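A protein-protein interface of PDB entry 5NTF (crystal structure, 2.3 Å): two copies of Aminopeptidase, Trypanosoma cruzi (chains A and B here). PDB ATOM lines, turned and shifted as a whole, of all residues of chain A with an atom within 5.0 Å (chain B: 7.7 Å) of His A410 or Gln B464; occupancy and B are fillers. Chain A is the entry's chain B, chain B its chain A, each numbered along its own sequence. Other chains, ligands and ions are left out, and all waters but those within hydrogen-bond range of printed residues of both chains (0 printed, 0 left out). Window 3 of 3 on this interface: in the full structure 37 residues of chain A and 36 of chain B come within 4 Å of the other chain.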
ATOM      1  N   GLY A 405      11.312 -20.969  -1.157  1.00  0.00           N
ATOM      2  CA  GLY A 405      12.207 -21.230  -0.041  1.00  0.00           C
ATOM      3  C   GLY A 405      11.419 -21.394   1.230  1.00  0.00           C
ATOM      4  O   GLY A 405      11.654 -22.316   2.019  1.00  0.00           O
ATOM      5  N   THR A 408       9.340 -25.042   0.747  1.00  0.00           N
ATOM      6  CA  THR A 408      10.118 -26.286   0.658  1.00  0.00           C
ATOM      7  C   THR A 408      11.637 -26.166   0.938  1.00  0.00           C
ATOM      8  O   THR A 408      12.363 -27.154   0.848  1.00  0.00           O
ATOM      9  CB  THR A 408       9.895 -26.988  -0.698  1.00  0.00           C
ATOM     10  OG1 THR A 408      10.451 -26.211  -1.751  1.00  0.00           O
ATOM     11  CG2 THR A 408       8.402 -27.240  -0.962  1.00  0.00           C
ATOM     12  N   GLY A 409      12.106 -24.984   1.311  1.00  0.00           N
ATOM     13  CA  GLY A 409      13.480 -24.825   1.782  1.00  0.00           C
ATOM     14  C   GLY A 409      14.517 -24.671   0.684  1.00  0.00           C
ATOM     15  O   GLY A 409      14.199 -24.631  -0.511  1.00  0.00           O
ATOM     16  N   HIS A 410      15.766 -24.610   1.114  1.00  0.00           N
ATOM     17  CA  HIS A 410      16.910 -24.341   0.227  1.00  0.00           C
ATOM     18  C   HIS A 410      17.336 -25.484  -0.673  1.00  0.00           C
ATOM     19  O   HIS A 410      17.897 -25.232  -1.730  1.00  0.00           O
ATOM     20  CB  HIS A 410      18.120 -23.888   1.049  1.00  0.00           C
ATOM     21  CG  HIS A 410      17.996 -22.488   1.561  1.00  0.00           C
ATOM     22  ND1 HIS A 410      19.084 -21.698   1.860  1.00  0.00           N
ATOM     23  CD2 HIS A 410      16.902 -21.722   1.788  1.00  0.00           C
ATOM     24  CE1 HIS A 410      18.666 -20.512   2.271  1.00  0.00           C
ATOM     25  NE2 HIS A 410      17.345 -20.498   2.234  1.00  0.00           N
ATOM     26  N   ARG A 411      17.098 -26.714  -0.232  1.00  0.00           N
ATOM     27  CA  ARG A 411      17.574 -27.904  -0.938  1.00  0.00           C
ATOM     28  C   ARG A 411      16.499 -28.727  -1.633  1.00  0.00           C
ATOM     29  O   ARG A 411      16.821 -29.629  -2.355  1.00  0.00           O
ATOM     30  CB  ARG A 411      18.427 -28.786  -0.029  1.00  0.00           C
ATOM     31  CG  ARG A 411      19.802 -28.176   0.252  1.00  0.00           C
ATOM     32  CD  ARG A 411      20.875 -29.210   0.581  1.00  0.00           C
ATOM     33  NE  ARG A 411      22.210 -28.611   0.697  1.00  0.00           N
ATOM     34  CZ  ARG A 411      22.615 -27.817   1.707  1.00  0.00           C
ATOM     35  NH1 ARG A 411      21.808 -27.487   2.732  1.00  0.00           N
ATOM     36  NH2 ARG A 411      23.852 -27.320   1.700  1.00  0.00           N
ATOM     37  N   HIS A 412      15.229 -28.417  -1.439  1.00  0.00           N
ATOM     38  CA  HIS A 412      14.155 -29.149  -2.093  1.00  0.00           C
ATOM     39  C   HIS A 412      13.344 -28.245  -3.000  1.00  0.00           C
ATOM     40  O   HIS A 412      12.657 -27.339  -2.528  1.00  0.00           O
ATOM     41  CB  HIS A 412      13.226 -29.774  -1.081  1.00  0.00           C
ATOM     42  CG  HIS A 412      13.834 -30.876  -0.288  1.00  0.00           C
ATOM     43  ND1 HIS A 412      14.579 -30.651   0.843  1.00  0.00           N
ATOM     44  CD2 HIS A 412      13.772 -32.218  -0.437  1.00  0.00           C
ATOM     45  CE1 HIS A 412      14.965 -31.809   1.351  1.00  0.00           C
ATOM     46  NE2 HIS A 412      14.477 -32.775   0.598  1.00  0.00           N
ATOM     47  N   PHE A 496      15.786 -21.510  -4.892  1.00  0.00           N
ATOM     48  CA  PHE A 496      16.888 -21.680  -3.921  1.00  0.00           C
ATOM     49  C   PHE A 496      17.812 -22.878  -4.122  1.00  0.00           C
ATOM     50  O   PHE A 496      18.999 -22.793  -3.808  1.00  0.00           O
ATOM     51  CB  PHE A 496      16.357 -21.734  -2.489  1.00  0.00           C
ATOM     52  CG  PHE A 496      15.944 -20.408  -1.976  1.00  0.00           C
ATOM     53  CD1 PHE A 496      14.656 -19.947  -2.191  1.00  0.00           C
ATOM     54  CD2 PHE A 496      16.846 -19.593  -1.330  1.00  0.00           C
ATOM     55  CE1 PHE A 496      14.268 -18.701  -1.742  1.00  0.00           C
ATOM     56  CE2 PHE A 496      16.463 -18.345  -0.865  1.00  0.00           C
ATOM     57  CZ  PHE A 496      15.167 -17.899  -1.076  1.00  0.00           C
ATOM     58  N   PRO A 497      17.283 -24.006  -4.599  1.00  0.00           N
ATOM     59  CA  PRO A 497      18.217 -25.112  -4.868  1.00  0.00           C
ATOM     60  C   PRO A 497      19.293 -24.811  -5.924  1.00  0.00           C
ATOM     61  O   PRO A 497      20.376 -25.388  -5.892  1.00  0.00           O
ATOM     62  CB  PRO A 497      17.291 -26.244  -5.353  1.00  0.00           C
ATOM     63  CG  PRO A 497      15.960 -25.924  -4.749  1.00  0.00           C
ATOM     64  CD  PRO A 497      15.875 -24.419  -4.712  1.00  0.00           C
ATOM     65  N   LEU B 441       7.527 -30.443   4.179  1.00  0.00           N
ATOM     66  CA  LEU B 441       8.814 -31.140   4.160  1.00  0.00           C
ATOM     67  C   LEU B 441       9.166 -31.738   5.504  1.00  0.00           C
ATOM     68  O   LEU B 441       9.257 -31.001   6.495  1.00  0.00           O
ATOM     69  CB  LEU B 441       9.927 -30.167   3.765  1.00  0.00           C
ATOM     70  CG  LEU B 441      11.339 -30.765   3.681  1.00  0.00           C
ATOM     71  CD1 LEU B 441      11.395 -31.878   2.636  1.00  0.00           C
ATOM     72  CD2 LEU B 441      12.377 -29.694   3.354  1.00  0.00           C
ATOM     73  N   TYR B 446      18.154 -31.109   7.818  1.00  0.00           N
ATOM     74  CA  TYR B 446      18.247 -29.718   7.348  1.00  0.00           C
ATOM     75  C   TYR B 446      17.645 -28.685   8.308  1.00  0.00           C
ATOM     76  O   TYR B 446      18.181 -27.575   8.430  1.00  0.00           O
ATOM     77  CB  TYR B 446      17.621 -29.544   5.959  1.00  0.00           C
ATOM     78  CG  TYR B 446      18.310 -30.325   4.872  1.00  0.00           C
ATOM     79  CD1 TYR B 446      19.601 -30.874   5.059  1.00  0.00           C
ATOM     80  CD2 TYR B 446      17.701 -30.493   3.619  1.00  0.00           C
ATOM     81  CE1 TYR B 446      20.213 -31.635   4.056  1.00  0.00           C
ATOM     82  CE2 TYR B 446      18.324 -31.210   2.600  1.00  0.00           C
ATOM     83  CZ  TYR B 446      19.581 -31.784   2.820  1.00  0.00           C
ATOM     84  OH  TYR B 446      20.210 -32.480   1.819  1.00  0.00           O
ATOM     85  N   THR B 449      19.711 -27.237  11.864  1.00  0.00           N
ATOM     86  CA  THR B 449      20.810 -26.272  11.685  1.00  0.00           C
ATOM     87  C   THR B 449      20.327 -24.823  11.754  1.00  0.00           C
ATOM     88  O   THR B 449      21.090 -23.919  12.125  1.00  0.00           O
ATOM     89  CB  THR B 449      21.507 -26.504  10.327  1.00  0.00           C
ATOM     90  OG1 THR B 449      20.526 -26.547   9.289  1.00  0.00           O
ATOM     91  CG2 THR B 449      22.249 -27.825  10.346  1.00  0.00           C
ATOM     92  N   GLU B 450      19.043 -24.628  11.433  1.00  0.00           N
ATOM     93  CA  GLU B 450      18.359 -23.347  11.622  1.00  0.00           C
ATOM     94  C   GLU B 450      18.235 -22.850  13.077  1.00  0.00           C
ATOM     95  O   GLU B 450      17.953 -21.681  13.294  1.00  0.00           O
ATOM     96  CB  GLU B 450      16.968 -23.383  10.969  1.00  0.00           C
ATOM     97  CG  GLU B 450      17.007 -23.454   9.453  1.00  0.00           C
ATOM     98  CD  GLU B 450      17.685 -22.242   8.839  1.00  0.00           C
ATOM     99  OE1 GLU B 450      17.692 -21.139   9.458  1.00  0.00           O
ATOM    100  OE2 GLU B 450      18.228 -22.359   7.715  1.00  0.00           O
ATOM    101  N   PHE B 451      18.442 -23.719  14.057  1.00  0.00           N
ATOM    102  CA  PHE B 451      18.315 -23.332  15.479  1.00  0.00           C
ATOM    103  C   PHE B 451      19.633 -23.321  16.262  1.00  0.00           C
ATOM    104  O   PHE B 451      19.616 -23.417  17.480  1.00  0.00           O
ATOM    105  CB  PHE B 451      17.305 -24.250  16.176  1.00  0.00           C
ATOM    106  CG  PHE B 451      15.905 -24.145  15.622  1.00  0.00           C
ATOM    107  CD1 PHE B 451      15.161 -22.976  15.767  1.00  0.00           C
ATOM    108  CD2 PHE B 451      15.313 -25.221  14.944  1.00  0.00           C
ATOM    109  CE1 PHE B 451      13.853 -22.890  15.255  1.00  0.00           C
ATOM    110  CE2 PHE B 451      14.015 -25.123  14.421  1.00  0.00           C
ATOM    111  CZ  PHE B 451      13.289 -23.955  14.581  1.00  0.00           C
ATOM    112  N   SER B 461      13.882 -19.456  17.129  1.00  0.00           N
ATOM    113  CA  SER B 461      13.427 -18.889  15.859  1.00  0.00           C
ATOM    114  C   SER B 461      14.507 -19.075  14.807  1.00  0.00           C
ATOM    115  O   SER B 461      15.682 -18.912  15.077  1.00  0.00           O
ATOM    116  CB  SER B 461      13.082 -17.404  16.021  1.00  0.00           C
ATOM    117  OG  SER B 461      12.441 -16.882  14.858  1.00  0.00           O
ATOM    118  N   VAL B 462      14.080 -19.394  13.601  1.00  0.00           N
ATOM    119  CA  VAL B 462      14.993 -19.759  12.510  1.00  0.00           C
ATOM    120  C   VAL B 462      15.942 -18.620  12.148  1.00  0.00           C
ATOM    121  O   VAL B 462      15.574 -17.462  12.209  1.00  0.00           O
ATOM    122  CB  VAL B 462      14.240 -20.207  11.228  1.00  0.00           C
ATOM    123  CG1 VAL B 462      13.451 -21.478  11.497  1.00  0.00           C
ATOM    124  CG2 VAL B 462      13.323 -19.128  10.689  1.00  0.00           C
ATOM    125  N   LYS B 463      17.166 -18.970  11.787  1.00  0.00           N
ATOM    126  CA  LYS B 463      18.147 -17.990  11.315  1.00  0.00           C
ATOM    127  C   LYS B 463      17.705 -17.451   9.971  1.00  0.00           C
ATOM    128  O   LYS B 463      17.710 -16.270   9.765  1.00  0.00           O
ATOM    129  CB  LYS B 463      19.559 -18.609  11.178  1.00  0.00           C
ATOM    130  N   GLN B 464      17.332 -18.348   9.068  1.00  0.00           N
ATOM    131  CA  GLN B 464      16.790 -17.986   7.744  1.00  0.00           C
ATOM    132  C   GLN B 464      15.270 -18.235   7.692  1.00  0.00           C
ATOM    133  O   GLN B 464      14.765 -19.331   8.010  1.00  0.00           O
ATOM    134  CB  GLN B 464      17.486 -18.771   6.634  1.00  0.00           C
ATOM    135  CG  GLN B 464      18.999 -18.540   6.568  1.00  0.00           C
ATOM    136  CD  GLN B 464      19.740 -19.616   5.792  1.00  0.00           C
ATOM    137  OE1 GLN B 464      20.383 -19.325   4.777  1.00  0.00           O
ATOM    138  NE2 GLN B 464      19.657 -20.873   6.262  1.00  0.00           N
ATOM    139  N   VAL B 465      14.563 -17.187   7.303  1.00  0.00           N
ATOM    140  CA  VAL B 465      13.114 -17.221   7.183  1.00  0.00           C
ATOM    141  C   VAL B 465      12.667 -18.002   5.945  1.00  0.00           C
ATOM    142  O   VAL B 465      11.629 -18.680   5.958  1.00  0.00           O
ATOM    143  CB  VAL B 465      12.519 -15.792   7.119  1.00  0.00           C
ATOM    144  CG1 VAL B 465      12.686 -15.101   8.473  1.00  0.00           C
ATOM    145  CG2 VAL B 465      13.120 -14.954   5.981  1.00  0.00           C
ATOM    146  N   ASN B 466      13.503 -17.934   4.916  1.00  0.00           N
ATOM    147  CA  ASN B 466      13.287 -18.574   3.599  1.00  0.00           C
ATOM    148  C   ASN B 466      13.708 -20.072   3.461  1.00  0.00           C
ATOM    149  O   ASN B 466      14.194 -20.479   2.391  1.00  0.00           O
ATOM    150  CB  ASN B 466      13.990 -17.728   2.501  1.00  0.00           C
ATOM    151  CG  ASN B 466      15.447 -17.310   2.877  1.00  0.00           C
ATOM    152  OD1 ASN B 466      16.163 -17.985   3.626  1.00  0.00           O
ATOM    153  ND2 ASN B 466      15.876 -16.189   2.332  1.00  0.00           N
ATOM    154  N   ASN B 467      13.512 -20.880   4.511  1.00  0.00           N
ATOM    155  CA  ASN B 467      14.042 -22.245   4.510  1.00  0.00           C
ATOM    156  C   ASN B 467      13.126 -23.252   5.203  1.00  0.00           C
ATOM    157  O   ASN B 467      13.498 -23.845   6.223  1.00  0.00           O
ATOM    158  CB  ASN B 467      15.455 -22.288   5.105  1.00  0.00           C
ATOM    159  CG  ASN B 467      16.176 -23.622   4.845  1.00  0.00           C
ATOM    160  OD1 ASN B 467      15.892 -24.339   3.876  1.00  0.00           O
ATOM    161  ND2 ASN B 467      17.124 -23.948   5.706  1.00  0.00           N
ATOM    162  N   ALA B 468      11.934 -23.443   4.620  1.00  0.00           N
ATOM    163  CA  ALA B 468      11.016 -24.478   5.070  1.00  0.00           C
ATOM    164  C   ALA B 468      10.645 -24.195   6.507  1.00  0.00           C
ATOM    165  O   ALA B 468      10.902 -24.980   7.400  1.00  0.00           O
ATOM    166  CB  ALA B 468      11.665 -25.856   4.954  1.00  0.00           C
ATOM    167  N   SER B 469      10.080 -23.030   6.724  1.00  0.00           N
ATOM    168  CA  SER B 469       9.922 -22.508   8.094  1.00  0.00           C
ATOM    169  C   SER B 469       8.777 -23.155   8.870  1.00  0.00           C
ATOM    170  O   SER B 469       8.821 -23.209  10.086  1.00  0.00           O
ATOM    171  CB  SER B 469       9.807 -20.977   8.088  1.00  0.00           C
ATOM    172  OG  SER B 469       8.573 -20.575   7.539  1.00  0.00           O
ATOM    173  N   CYS B 472      10.448 -26.307  10.080  1.00  0.00           N
ATOM    174  CA  CYS B 472      11.355 -25.970  11.148  1.00  0.00           C
ATOM    175  C   CYS B 472      10.630 -25.850  12.477  1.00  0.00           C
ATOM    176  O   CYS B 472      11.087 -26.350  13.493  1.00  0.00           O
ATOM    177  CB  CYS B 472      12.164 -24.677  10.810  1.00  0.00           C
ATOM    178  SG  CYS B 472      13.407 -24.876   9.461  1.00  0.00           S
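Of the 8 printed residues of chain A, 7 touch a printed residue of chain B. Hydrophobic or aromatic side chains of chain A within 4 Å of the printed part of chain B: His A410, His A412 and Phe A496. Along chain A the printed residues that touch a printed residue of chain B span positions 405 to 496. Among the printed residues, 13 pairs touch across the chains.
The backbone carbonyl oxygen of Gly A405 sits at hydrogen-bond distance from the backbone NH of Asn B467 (3.4 Å). The side-chain amide oxygen (OD1) of Asn B466 lies within hydrogen-bond range of a ring nitrogen (NE2) of His A410. N of Ala B468 lies within hydrogen-bond range of O of Gly A405. N of His A410 lies within hydrogen-bond range of OD1 of Asn B467, 2.8 Å away. The backbone carbonyl oxygen of Gly A405 lies close to the backbone carbonyl oxygen of Asn B466.
No position is printed for both chains.
Gln B464 touches just one residue of chain A: His A410 (3.3 Å). Printed residues of chain A within 4 Å of Tyr B446: Arg A411 (3.6 Å) and His A412 (3.6 Å). Of the printed residues of chain B, Thr A408 touches Leu B441 (3.6 Å). Of the printed residues of chain B, Gly A405 touches Asn B466 (3.1 Å), Asn B467 (3.4 Å) and Ala B468 (2.8 Å). Of the printed residues of chain A, Asn B466 touches Gly A405 (3.1 Å), His A410 (3.0 Å) and Phe A496 (3.8 Å). Ser B469 touches none of the printed residues of chain A. Val B465 touches none of the printed residues of chain A. The nearest printed residue of chain A that does not touch Asn B467 is Arg A411 (4.9 Å).
Among the printed residues, pairs that only touch across the chains: Thr A408 with Leu B441 (3.6 Å), Gly A409 with Asn B467 (3.2 Å), Gly A409 with Ala B468 (3.5 Å), His A410 with Gln B464 (3.3 Å), Arg A411 with Tyr B446 (3.6 Å), His A412 with Leu B441 (3.5 Å), His A412 with Tyr B446 (3.6 Å) and Phe A496 with Asn B466 (3.8 Å).
O of His A412 sits at hydrogen-bond distance from OG1 of Thr A408 (2.6 Å). ND2 of Asn B467 is in hydrogen-bond range of OE2 of Glu B450 (2.8 Å). The backbone carbonyl oxygen of Tyr B446 sits at hydrogen-bond distance from the side-chain hydroxyl of Thr B449 (2.7 Å). The backbone carbonyl oxygen of Ala B468 is in hydrogen-bond range of the side-chain sulfur of Cys B472 (3.2 Å). OE2 of Glu B450 is in hydrogen-bond range of NE2 of Gln B464 (2.5 Å). The backbone carbonyl oxygen of Asn B467 lies within hydrogen-bond range of the side-chain sulfur of Cys B472, at 3.4 Å.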
